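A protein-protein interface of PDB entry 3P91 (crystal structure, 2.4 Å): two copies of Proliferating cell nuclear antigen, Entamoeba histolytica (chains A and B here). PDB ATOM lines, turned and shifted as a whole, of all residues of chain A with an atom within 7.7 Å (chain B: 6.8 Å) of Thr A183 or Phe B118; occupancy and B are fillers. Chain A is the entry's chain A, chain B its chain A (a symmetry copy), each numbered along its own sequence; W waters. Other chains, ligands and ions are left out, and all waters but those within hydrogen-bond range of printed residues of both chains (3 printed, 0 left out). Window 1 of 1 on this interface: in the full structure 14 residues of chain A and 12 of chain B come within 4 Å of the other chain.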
ATOM      1  N   ILE A 151      -1.328 -11.727 -31.666  1.00  0.00           N
ATOM      2  CA  ILE A 151      -0.779 -11.243 -30.423  1.00  0.00           C
ATOM      3  C   ILE A 151      -1.416  -9.930 -30.028  1.00  0.00           C
ATOM      4  O   ILE A 151      -1.855  -9.771 -28.898  1.00  0.00           O
ATOM      5  CB  ILE A 151       0.726 -11.078 -30.523  1.00  0.00           C
ATOM      6  CG1 ILE A 151       1.375 -12.438 -30.779  1.00  0.00           C
ATOM      7  CG2 ILE A 151       1.271 -10.452 -29.252  1.00  0.00           C
ATOM      8  CD1 ILE A 151       2.883 -12.387 -30.876  1.00  0.00           C
ATOM      9  N   ASP A 154      -4.875 -10.787 -28.615  1.00  0.00           N
ATOM     10  CA  ASP A 154      -4.922 -11.311 -27.261  1.00  0.00           C
ATOM     11  C   ASP A 154      -4.620 -10.195 -26.284  1.00  0.00           C
ATOM     12  O   ASP A 154      -5.287 -10.053 -25.267  1.00  0.00           O
ATOM     13  CB  ASP A 154      -3.911 -12.431 -27.086  1.00  0.00           C
ATOM     14  CG  ASP A 154      -4.215 -13.633 -27.952  1.00  0.00           C
ATOM     15  OD1 ASP A 154      -3.258 -14.359 -28.303  1.00  0.00           O
ATOM     16  OD2 ASP A 154      -5.402 -13.857 -28.276  1.00  0.00           O
ATOM     17  N   PHE A 155      -3.613  -9.396 -26.612  1.00  0.00           N
ATOM     18  CA  PHE A 155      -3.203  -8.276 -25.770  1.00  0.00           C
ATOM     19  C   PHE A 155      -4.296  -7.241 -25.527  1.00  0.00           C
ATOM     20  O   PHE A 155      -4.417  -6.721 -24.426  1.00  0.00           O
ATOM     21  CB  PHE A 155      -1.941  -7.615 -26.339  1.00  0.00           C
ATOM     22  CG  PHE A 155      -0.667  -8.245 -25.855  1.00  0.00           C
ATOM     23  CD1 PHE A 155      -0.521  -9.622 -25.846  1.00  0.00           C
ATOM     24  CD2 PHE A 155       0.381  -7.464 -25.399  1.00  0.00           C
ATOM     25  CE1 PHE A 155       0.648 -10.208 -25.388  1.00  0.00           C
ATOM     26  CE2 PHE A 155       1.553  -8.044 -24.942  1.00  0.00           C
ATOM     27  CZ  PHE A 155       1.687  -9.420 -24.942  1.00  0.00           C
ATOM     28  N   ALA A 157      -7.429  -7.827 -25.428  1.00  0.00           N
ATOM     29  CA  ALA A 157      -8.374  -8.463 -24.529  1.00  0.00           C
ATOM     30  C   ALA A 157      -7.859  -8.528 -23.098  1.00  0.00           C
ATOM     31  O   ALA A 157      -8.630  -8.384 -22.150  1.00  0.00           O
ATOM     32  CB  ALA A 157      -8.706  -9.862 -25.024  1.00  0.00           C
ATOM     33  N   LEU A 158      -6.558  -8.743 -22.947  1.00  0.00           N
ATOM     34  CA  LEU A 158      -5.972  -9.014 -21.643  1.00  0.00           C
ATOM     35  C   LEU A 158      -5.172  -7.844 -21.080  1.00  0.00           C
ATOM     36  O   LEU A 158      -4.792  -7.851 -19.907  1.00  0.00           O
ATOM     37  CB  LEU A 158      -5.063 -10.230 -21.745  1.00  0.00           C
ATOM     38  CG  LEU A 158      -5.707 -11.521 -22.232  1.00  0.00           C
ATOM     39  CD1 LEU A 158      -4.648 -12.529 -22.627  1.00  0.00           C
ATOM     40  CD2 LEU A 158      -6.646 -12.099 -21.173  1.00  0.00           C
ATOM     41  N   GLY A 159      -4.905  -6.845 -21.911  1.00  0.00           N
ATOM     42  CA  GLY A 159      -4.053  -5.749 -21.499  1.00  0.00           C
ATOM     43  C   GLY A 159      -4.798  -4.478 -21.161  1.00  0.00           C
ATOM     44  O   GLY A 159      -6.027  -4.449 -21.152  1.00  0.00           O
ATOM     45  N   THR A 164       4.507  -3.249 -24.365  1.00  0.00           N
ATOM     46  CA  THR A 164       5.941  -3.060 -24.367  1.00  0.00           C
ATOM     47  C   THR A 164       6.600  -4.068 -25.285  1.00  0.00           C
ATOM     48  O   THR A 164       6.270  -5.247 -25.279  1.00  0.00           O
ATOM     49  CB  THR A 164       6.509  -3.154 -22.954  1.00  0.00           C
ATOM     50  OG1 THR A 164       6.067  -2.016 -22.204  1.00  0.00           O
ATOM     51  CG2 THR A 164       8.033  -3.188 -22.977  1.00  0.00           C
ATOM     52  N   THR A 173      10.438  -9.588 -26.980  1.00  0.00           N
ATOM     53  CA  THR A 173       9.611  -9.723 -25.802  1.00  0.00           C
ATOM     54  C   THR A 173       8.476  -8.722 -25.867  1.00  0.00           C
ATOM     55  O   THR A 173       8.689  -7.556 -26.183  1.00  0.00           O
ATOM     56  CB  THR A 173      10.435  -9.494 -24.537  1.00  0.00           C
ATOM     57  OG1 THR A 173      11.494 -10.458 -24.487  1.00  0.00           O
ATOM     58  CG2 THR A 173       9.568  -9.641 -23.302  1.00  0.00           C
ATOM     59  N   LEU A 174       7.265  -9.193 -25.594  1.00  0.00           N
ATOM     60  CA  LEU A 174       6.086  -8.357 -25.725  1.00  0.00           C
ATOM     61  C   LEU A 174       5.301  -8.431 -24.450  1.00  0.00           C
ATOM     62  O   LEU A 174       4.894  -9.506 -24.026  1.00  0.00           O
ATOM     63  CB  LEU A 174       5.222  -8.820 -26.890  1.00  0.00           C
ATOM     64  CG  LEU A 174       5.922  -8.861 -28.245  1.00  0.00           C
ATOM     65  CD1 LEU A 174       6.173 -10.299 -28.648  1.00  0.00           C
ATOM     66  CD2 LEU A 174       5.102  -8.164 -29.289  1.00  0.00           C
ATOM     67  N   THR A 175       5.080  -7.277 -23.844  1.00  0.00           N
ATOM     68  CA  THR A 175       4.491  -7.225 -22.523  1.00  0.00           C
ATOM     69  C   THR A 175       3.309  -6.263 -22.439  1.00  0.00           C
ATOM     70  O   THR A 175       3.354  -5.158 -22.974  1.00  0.00           O
ATOM     71  CB  THR A 175       5.558  -6.833 -21.493  1.00  0.00           C
ATOM     72  OG1 THR A 175       6.433  -7.945 -21.278  1.00  0.00           O
ATOM     73  CG2 THR A 175       4.924  -6.444 -20.174  1.00  0.00           C
ATOM     74  N   THR A 176       2.247  -6.714 -21.782  1.00  0.00           N
ATOM     75  CA  THR A 176       1.165  -5.843 -21.343  1.00  0.00           C
ATOM     76  C   THR A 176       0.656  -6.341 -19.986  1.00  0.00           C
ATOM     77  O   THR A 176       0.727  -7.534 -19.688  1.00  0.00           O
ATOM     78  CB  THR A 176       0.017  -5.753 -22.387  1.00  0.00           C
ATOM     79  OG1 THR A 176      -0.845  -4.654 -22.067  1.00  0.00           O
ATOM     80  CG2 THR A 176      -0.797  -7.029 -22.428  1.00  0.00           C
ATOM     81  N   LYS A 177       0.185  -5.416 -19.154  1.00  0.00           N
ATOM     82  CA  LYS A 177      -0.366  -5.741 -17.844  1.00  0.00           C
ATOM     83  C   LYS A 177      -1.748  -5.120 -17.723  1.00  0.00           C
ATOM     84  O   LYS A 177      -1.890  -3.902 -17.784  1.00  0.00           O
ATOM     85  CB  LYS A 177       0.542  -5.215 -16.727  1.00  0.00           C
ATOM     86  N   GLY A 178      -2.767  -5.959 -17.561  1.00  0.00           N
ATOM     87  CA  GLY A 178      -4.132  -5.490 -17.396  1.00  0.00           C
ATOM     88  C   GLY A 178      -4.610  -5.509 -15.954  1.00  0.00           C
ATOM     89  O   GLY A 178      -3.830  -5.713 -15.020  1.00  0.00           O
ATOM     90  N   MET A 180      -6.570  -7.626 -14.496  1.00  0.00           N
ATOM     91  CA  MET A 180      -6.626  -8.946 -13.888  1.00  0.00           C
ATOM     92  C   MET A 180      -5.521  -9.866 -14.374  1.00  0.00           C
ATOM     93  O   MET A 180      -5.487 -11.048 -14.020  1.00  0.00           O
ATOM     94  CB  MET A 180      -7.994  -9.587 -14.136  1.00  0.00           C
ATOM     95  CG  MET A 180      -8.469  -9.552 -15.582  1.00  0.00           C
ATOM     96  SD  MET A 180      -8.057 -11.014 -16.565  1.00  0.00           S
ATOM     97  CE  MET A 180      -9.015 -10.654 -18.045  1.00  0.00           C
ATOM     98  N   CYS A 181      -4.605  -9.324 -15.165  1.00  0.00           N
ATOM     99  CA  CYS A 181      -3.652 -10.169 -15.849  1.00  0.00           C
ATOM    100  C   CYS A 181      -2.368  -9.420 -16.162  1.00  0.00           C
ATOM    101  O   CYS A 181      -2.403  -8.249 -16.512  1.00  0.00           O
ATOM    102  CB  CYS A 181      -4.291 -10.674 -17.140  1.00  0.00           C
ATOM    103  SG  CYS A 181      -3.437 -12.025 -17.933  1.00  0.00           S
ATOM    104  N   GLU A 182      -1.234 -10.096 -16.012  1.00  0.00           N
ATOM    105  CA  GLU A 182       0.022  -9.610 -16.562  1.00  0.00           C
ATOM    106  C   GLU A 182       0.454 -10.622 -17.609  1.00  0.00           C
ATOM    107  O   GLU A 182       0.542 -11.811 -17.329  1.00  0.00           O
ATOM    108  CB  GLU A 182       1.091  -9.451 -15.480  1.00  0.00           C
ATOM    109  N   THR A 183       0.696 -10.153 -18.826  1.00  0.00           N
ATOM    110  CA  THR A 183       0.968 -11.053 -19.936  1.00  0.00           C
ATOM    111  C   THR A 183       2.346 -10.825 -20.528  1.00  0.00           C
ATOM    112  O   THR A 183       2.839  -9.706 -20.566  1.00  0.00           O
ATOM    113  CB  THR A 183      -0.078 -10.896 -21.040  1.00  0.00           C
ATOM    114  OG1 THR A 183      -1.388 -11.037 -20.477  1.00  0.00           O
ATOM    115  CG2 THR A 183       0.124 -11.940 -22.119  1.00  0.00           C
ATOM    116  N   CYS A 184       2.958 -11.906 -20.992  1.00  0.00           N
ATOM    117  CA  CYS A 184       4.286 -11.848 -21.563  1.00  0.00           C
ATOM    118  C   CYS A 184       4.445 -12.921 -22.630  1.00  0.00           C
ATOM    119  O   CYS A 184       4.413 -14.109 -22.323  1.00  0.00           O
ATOM    120  CB  CYS A 184       5.325 -12.068 -20.467  1.00  0.00           C
ATOM    121  SG  CYS A 184       7.032 -11.931 -21.037  1.00  0.00           S
ATOM    122  N   MET A 185       4.596 -12.495 -23.883  1.00  0.00           N
ATOM    123  CA  MET A 185       4.932 -13.404 -24.978  1.00  0.00           C
ATOM    124  C   MET A 185       6.409 -13.245 -25.298  1.00  0.00           C
ATOM    125  O   MET A 185       6.932 -12.134 -25.320  1.00  0.00           O
ATOM    126  CB  MET A 185       4.080 -13.135 -26.231  1.00  0.00           C
ATOM    127  N   LYS B  82     -10.774 -16.238 -20.733  1.00  0.00           N
ATOM    128  CA  LYS B  82     -10.120 -15.226 -21.566  1.00  0.00           C
ATOM    129  C   LYS B  82      -8.628 -15.516 -21.787  1.00  0.00           C
ATOM    130  O   LYS B  82      -8.105 -15.344 -22.884  1.00  0.00           O
ATOM    131  CB  LYS B  82     -10.319 -13.824 -20.978  1.00  0.00           C
ATOM    132  CG  LYS B  82     -11.770 -13.355 -21.009  1.00  0.00           C
ATOM    133  CD  LYS B  82     -11.925 -11.910 -20.566  1.00  0.00           C
ATOM    134  CE  LYS B  82     -11.373 -10.954 -21.597  1.00  0.00           C
ATOM    135  NZ  LYS B  82     -11.591  -9.534 -21.208  1.00  0.00           N
ATOM    136  N   ILE B  83      -7.947 -15.968 -20.744  1.00  0.00           N
ATOM    137  CA  ILE B  83      -6.555 -16.370 -20.880  1.00  0.00           C
ATOM    138  C   ILE B  83      -6.406 -17.643 -21.712  1.00  0.00           C
ATOM    139  O   ILE B  83      -5.558 -17.719 -22.600  1.00  0.00           O
ATOM    140  CB  ILE B  83      -5.903 -16.592 -19.511  1.00  0.00           C
ATOM    141  CG1 ILE B  83      -6.026 -15.333 -18.657  1.00  0.00           C
ATOM    142  CG2 ILE B  83      -4.460 -16.983 -19.677  1.00  0.00           C
ATOM    143  CD1 ILE B  83      -5.401 -15.464 -17.281  1.00  0.00           C
ATOM    144  N   LEU B  84      -7.239 -18.640 -21.415  1.00  0.00           N
ATOM    145  CA  LEU B  84      -7.174 -19.940 -22.079  1.00  0.00           C
ATOM    146  C   LEU B  84      -7.556 -19.877 -23.552  1.00  0.00           C
ATOM    147  O   LEU B  84      -7.049 -20.640 -24.370  1.00  0.00           O
ATOM    148  CB  LEU B  84      -8.071 -20.939 -21.360  1.00  0.00           C
ATOM    149  CG  LEU B  84      -7.605 -21.277 -19.954  1.00  0.00           C
ATOM    150  CD1 LEU B  84      -8.331 -22.502 -19.464  1.00  0.00           C
ATOM    151  CD2 LEU B  84      -6.106 -21.503 -19.979  1.00  0.00           C
ATOM    152  N   ALA B  86      -6.663 -17.751 -25.502  1.00  0.00           N
ATOM    153  CA  ALA B  86      -5.495 -17.269 -26.226  1.00  0.00           C
ATOM    154  C   ALA B  86      -4.540 -18.394 -26.593  1.00  0.00           C
ATOM    155  O   ALA B  86      -3.593 -18.192 -27.349  1.00  0.00           O
ATOM    156  CB  ALA B  86      -4.768 -16.207 -25.416  1.00  0.00           C
ATOM    157  N   LEU B  87      -4.789 -19.580 -26.059  1.00  0.00           N
ATOM    158  CA  LEU B  87      -3.867 -20.690 -26.238  1.00  0.00           C
ATOM    159  C   LEU B  87      -4.345 -21.617 -27.337  1.00  0.00           C
ATOM    160  O   LEU B  87      -5.509 -21.576 -27.724  1.00  0.00           O
ATOM    161  CB  LEU B  87      -3.717 -21.463 -24.930  1.00  0.00           C
ATOM    162  CG  LEU B  87      -2.903 -20.804 -23.813  1.00  0.00           C
ATOM    163  CD1 LEU B  87      -3.191 -19.320 -23.684  1.00  0.00           C
ATOM    164  CD2 LEU B  87      -3.162 -21.503 -22.503  1.00  0.00           C
ATOM    165  N   LEU B  93       0.719 -26.653 -21.680  1.00  0.00           N
ATOM    166  CA  LEU B  93       0.131 -25.792 -20.668  1.00  0.00           C
ATOM    167  C   LEU B  93       0.625 -26.134 -19.263  1.00  0.00           C
ATOM    168  O   LEU B  93       0.517 -27.273 -18.808  1.00  0.00           O
ATOM    169  CB  LEU B  93      -1.395 -25.852 -20.741  1.00  0.00           C
ATOM    170  CG  LEU B  93      -2.117 -24.988 -19.713  1.00  0.00           C
ATOM    171  CD1 LEU B  93      -1.894 -23.524 -20.000  1.00  0.00           C
ATOM    172  CD2 LEU B  93      -3.588 -25.302 -19.706  1.00  0.00           C
ATOM    173  N   ALA B 103      -1.355 -15.246  -7.106  1.00  0.00           N
ATOM    174  CA  ALA B 103      -1.316 -15.296  -8.566  1.00  0.00           C
ATOM    175  C   ALA B 103      -1.020 -16.700  -9.087  1.00  0.00           C
ATOM    176  O   ALA B 103      -0.078 -17.350  -8.640  1.00  0.00           O
ATOM    177  CB  ALA B 103      -0.290 -14.291  -9.123  1.00  0.00           C
ATOM    178  N   VAL B 104      -1.834 -17.162 -10.030  1.00  0.00           N
ATOM    179  CA  VAL B 104      -1.577 -18.417 -10.720  1.00  0.00           C
ATOM    180  C   VAL B 104      -0.942 -18.157 -12.083  1.00  0.00           C
ATOM    181  O   VAL B 104      -1.516 -17.496 -12.953  1.00  0.00           O
ATOM    182  CB  VAL B 104      -2.862 -19.258 -10.891  1.00  0.00           C
ATOM    183  CG1 VAL B 104      -4.015 -18.370 -11.264  1.00  0.00           C
ATOM    184  CG2 VAL B 104      -2.665 -20.366 -11.933  1.00  0.00           C
ATOM    185  N   LEU B 105       0.256 -18.689 -12.258  1.00  0.00           N
ATOM    186  CA  LEU B 105       0.982 -18.506 -13.493  1.00  0.00           C
ATOM    187  C   LEU B 105       0.633 -19.584 -14.488  1.00  0.00           C
ATOM    188  O   LEU B 105       0.889 -20.758 -14.240  1.00  0.00           O
ATOM    189  CB  LEU B 105       2.473 -18.531 -13.216  1.00  0.00           C
ATOM    190  CG  LEU B 105       2.853 -17.372 -12.311  1.00  0.00           C
ATOM    191  CD1 LEU B 105       4.130 -17.683 -11.525  1.00  0.00           C
ATOM    192  CD2 LEU B 105       2.966 -16.069 -13.135  1.00  0.00           C
ATOM    193  N   SER B 106       0.048 -19.171 -15.612  1.00  0.00           N
ATOM    194  CA  SER B 106      -0.207 -20.071 -16.729  1.00  0.00           C
ATOM    195  C   SER B 106       0.887 -19.880 -17.770  1.00  0.00           C
ATOM    196  O   SER B 106       1.281 -18.755 -18.072  1.00  0.00           O
ATOM    197  CB  SER B 106      -1.581 -19.806 -17.360  1.00  0.00           C
ATOM    198  OG  SER B 106      -2.585 -19.646 -16.370  1.00  0.00           O
ATOM    199  N   ILE B 107       1.376 -20.980 -18.324  1.00  0.00           N
ATOM    200  CA  ILE B 107       2.445 -20.893 -19.300  1.00  0.00           C
ATOM    201  C   ILE B 107       2.221 -21.783 -20.517  1.00  0.00           C
ATOM    202  O   ILE B 107       2.001 -22.984 -20.389  1.00  0.00           O
ATOM    203  CB  ILE B 107       3.790 -21.216 -18.661  1.00  0.00           C
ATOM    204  CG1 ILE B 107       4.111 -20.163 -17.604  1.00  0.00           C
ATOM    205  CG2 ILE B 107       4.871 -21.287 -19.719  1.00  0.00           C
ATOM    206  CD1 ILE B 107       5.544 -20.158 -17.157  1.00  0.00           C
ATOM    207  N   THR B 108       2.266 -21.164 -21.695  1.00  0.00           N
ATOM    208  CA  THR B 108       2.202 -21.866 -22.972  1.00  0.00           C
ATOM    209  C   THR B 108       3.596 -21.978 -23.567  1.00  0.00           C
ATOM    210  O   THR B 108       4.282 -20.974 -23.725  1.00  0.00           O
ATOM    211  CB  THR B 108       1.355 -21.093 -23.995  1.00  0.00           C
ATOM    212  OG1 THR B 108      -0.012 -21.078 -23.585  1.00  0.00           O
ATOM    213  CG2 THR B 108       1.459 -21.730 -25.372  1.00  0.00           C
ATOM    214  N   MET B 116       4.298 -18.061 -23.772  1.00  0.00           N
ATOM    215  CA  MET B 116       3.434 -17.054 -23.191  1.00  0.00           C
ATOM    216  C   MET B 116       3.283 -17.289 -21.697  1.00  0.00           C
ATOM    217  O   MET B 116       3.014 -18.403 -21.256  1.00  0.00           O
ATOM    218  CB  MET B 116       2.078 -17.078 -23.890  1.00  0.00           C
ATOM    219  CG  MET B 116       2.183 -16.907 -25.402  1.00  0.00           C
ATOM    220  SD  MET B 116       0.647 -17.219 -26.297  1.00  0.00           S
ATOM    221  CE  MET B 116      -0.410 -15.955 -25.605  1.00  0.00           C
ATOM    222  N   LYS B 117       3.480 -16.241 -20.909  1.00  0.00           N
ATOM    223  CA  LYS B 117       3.324 -16.363 -19.476  1.00  0.00           C
ATOM    224  C   LYS B 117       2.296 -15.361 -19.002  1.00  0.00           C
ATOM    225  O   LYS B 117       2.377 -14.176 -19.307  1.00  0.00           O
ATOM    226  CB  LYS B 117       4.655 -16.141 -18.756  1.00  0.00           C
ATOM    227  N   PHE B 118       1.317 -15.849 -18.260  1.00  0.00           N
ATOM    228  CA  PHE B 118       0.300 -14.982 -17.702  1.00  0.00           C
ATOM    229  C   PHE B 118       0.347 -15.081 -16.197  1.00  0.00           C
ATOM    230  O   PHE B 118       0.558 -16.157 -15.648  1.00  0.00           O
ATOM    231  CB  PHE B 118      -1.082 -15.406 -18.180  1.00  0.00           C
ATOM    232  CG  PHE B 118      -1.126 -15.810 -19.621  1.00  0.00           C
ATOM    233  CD1 PHE B 118      -1.636 -14.954 -20.580  1.00  0.00           C
ATOM    234  CD2 PHE B 118      -0.660 -17.052 -20.021  1.00  0.00           C
ATOM    235  CE1 PHE B 118      -1.681 -15.325 -21.905  1.00  0.00           C
ATOM    236  CE2 PHE B 118      -0.700 -17.429 -21.348  1.00  0.00           C
ATOM    237  CZ  PHE B 118      -1.212 -16.568 -22.288  1.00  0.00           C
ATOM    238  N   GLY B 119       0.170 -13.947 -15.534  1.00  0.00           N
ATOM    239  CA  GLY B 119      -0.091 -13.929 -14.112  1.00  0.00           C
ATOM    240  C   GLY B 119      -1.562 -13.619 -13.920  1.00  0.00           C
ATOM    241  O   GLY B 119      -2.001 -12.505 -14.181  1.00  0.00           O
ATOM    242  N   LEU B 120      -2.330 -14.612 -13.492  1.00  0.00           N
ATOM    243  CA  LEU B 120      -3.734 -14.397 -13.176  1.00  0.00           C
ATOM    244  C   LEU B 120      -3.910 -14.088 -11.696  1.00  0.00           C
ATOM    245  O   LEU B 120      -3.519 -14.878 -10.844  1.00  0.00           O
ATOM    246  CB  LEU B 120      -4.559 -15.628 -13.527  1.00  0.00           C
ATOM    247  CG  LEU B 120      -5.961 -15.621 -12.910  1.00  0.00           C
ATOM    248  CD1 LEU B 120      -6.757 -14.400 -13.374  1.00  0.00           C
ATOM    249  CD2 LEU B 120      -6.701 -16.908 -13.235  1.00  0.00           C
HETATM  250  O   HOH W   1      -1.070 -10.417 -12.602  1.00  0.00           O
HETATM  251  O   HOH W   2      -0.158 -14.685 -28.922  1.00  0.00           O
HETATM  252  O   HOH W   3       3.800 -12.950 -16.919  1.00  0.00           O
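The side-chain amino group (NZ) of Lys B82 sits at hydrogen-bond distance from the backbone carbonyl oxygen (O) of Ala A157, 3.3 Å away. O of Cys A184 lies within hydrogen-bond range of N of Lys B117, 2.7 Å away. O of Glu A182 is in hydrogen-bond range of N of Gly B119, at 2.8 Å.
Water W1 lies within hydrogen-bond range of the backbone carbonyl oxygen of Gly B119 (2.8 Å) and the backbone NH of Glu A182 (3.4 Å). Water W3 lies within hydrogen-bond range of the backbone carbonyl oxygen (O) of Lys B117 (3.0 Å) and the backbone carbonyl oxygen (O) of Glu A182 (3.5 Å). Water W2 lies within hydrogen-bond range of OD1 of Asp A154 and SD of Met B116.
Asp A154 touches Ala B86 (CG to CB, 3.7 Å). Leu A158 touches Lys B82 (CD2 to O, 3.9 Å). O of Met A180 touches O of Gly B119, at 3.8 Å. Met A180 touches Leu B120. Gly B119 touches Cys A181 (O to CA, 3.3 Å). Lys B117 touches Glu A182. Phe B118 touches Glu A182. CA of Thr A183 touches O of Lys B117, at 3.5 Å. Thr A183 touches Phe B118 (CG2 to CD1, 3.8 Å). Cys A184 touches Met B116.
No position is printed for both chains.
Gly A178 touches none of the printed residues of chain B. Thr A183 touches just these residues of chain B: Lys B117 (3.5 Å) and Phe B118 (3.8 Å). Of the printed residues of chain A, Ala B86 touches Asp A154 (3.7 Å). Of the printed residues of chain A, Met B116 touches Cys A184. Lys B117 touches just these residues of chain A: Glu A182, Thr A183 and Cys A184. Phe B118 touches two residues of chain A. The nearest residue of chain B that does not touch Thr A183 is Gly B119 (5.1 Å).
The backbone carbonyl oxygen (O) of Met B116 is in hydrogen-bond range of the backbone NH (N) of Thr B108 (2.9 Å). The backbone carbonyl oxygen (O) of Leu B120 sits at hydrogen-bond distance from the backbone NH (N) of Val B104. O of Ser B106 sits at hydrogen-bond distance from N of Phe B118 (2.9 Å). SG of Cys A181 lies within hydrogen-bond range of OG1 of Thr A183, 3.4 Å away. The backbone NH (N) of Thr A183 is in hydrogen-bond range of the backbone carbonyl oxygen (O) of Thr A176.
Hydrophobic or aromatic side chains of chain A that line the printed part of chain B: Leu A158. Of the 17 printed residues of chain B, 7 touch a printed residue of chain A. Printed residues of chain B that touch a printed residue of chain A: Lys B82, Ala B86, Met B116, Lys B117, Phe B118, Gly B119 and Leu B120. Hydrophobic or aromatic side chains of chain B that line the printed part of chain A: Ala B86, Phe B118 and Leu B120. Among the printed residues, 13 pairs touch across the chains. Among the printed residues, no Asp or Glu carboxylate lies within 4 Å of a Lys or Arg side-chain nitrogen of the other chain.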
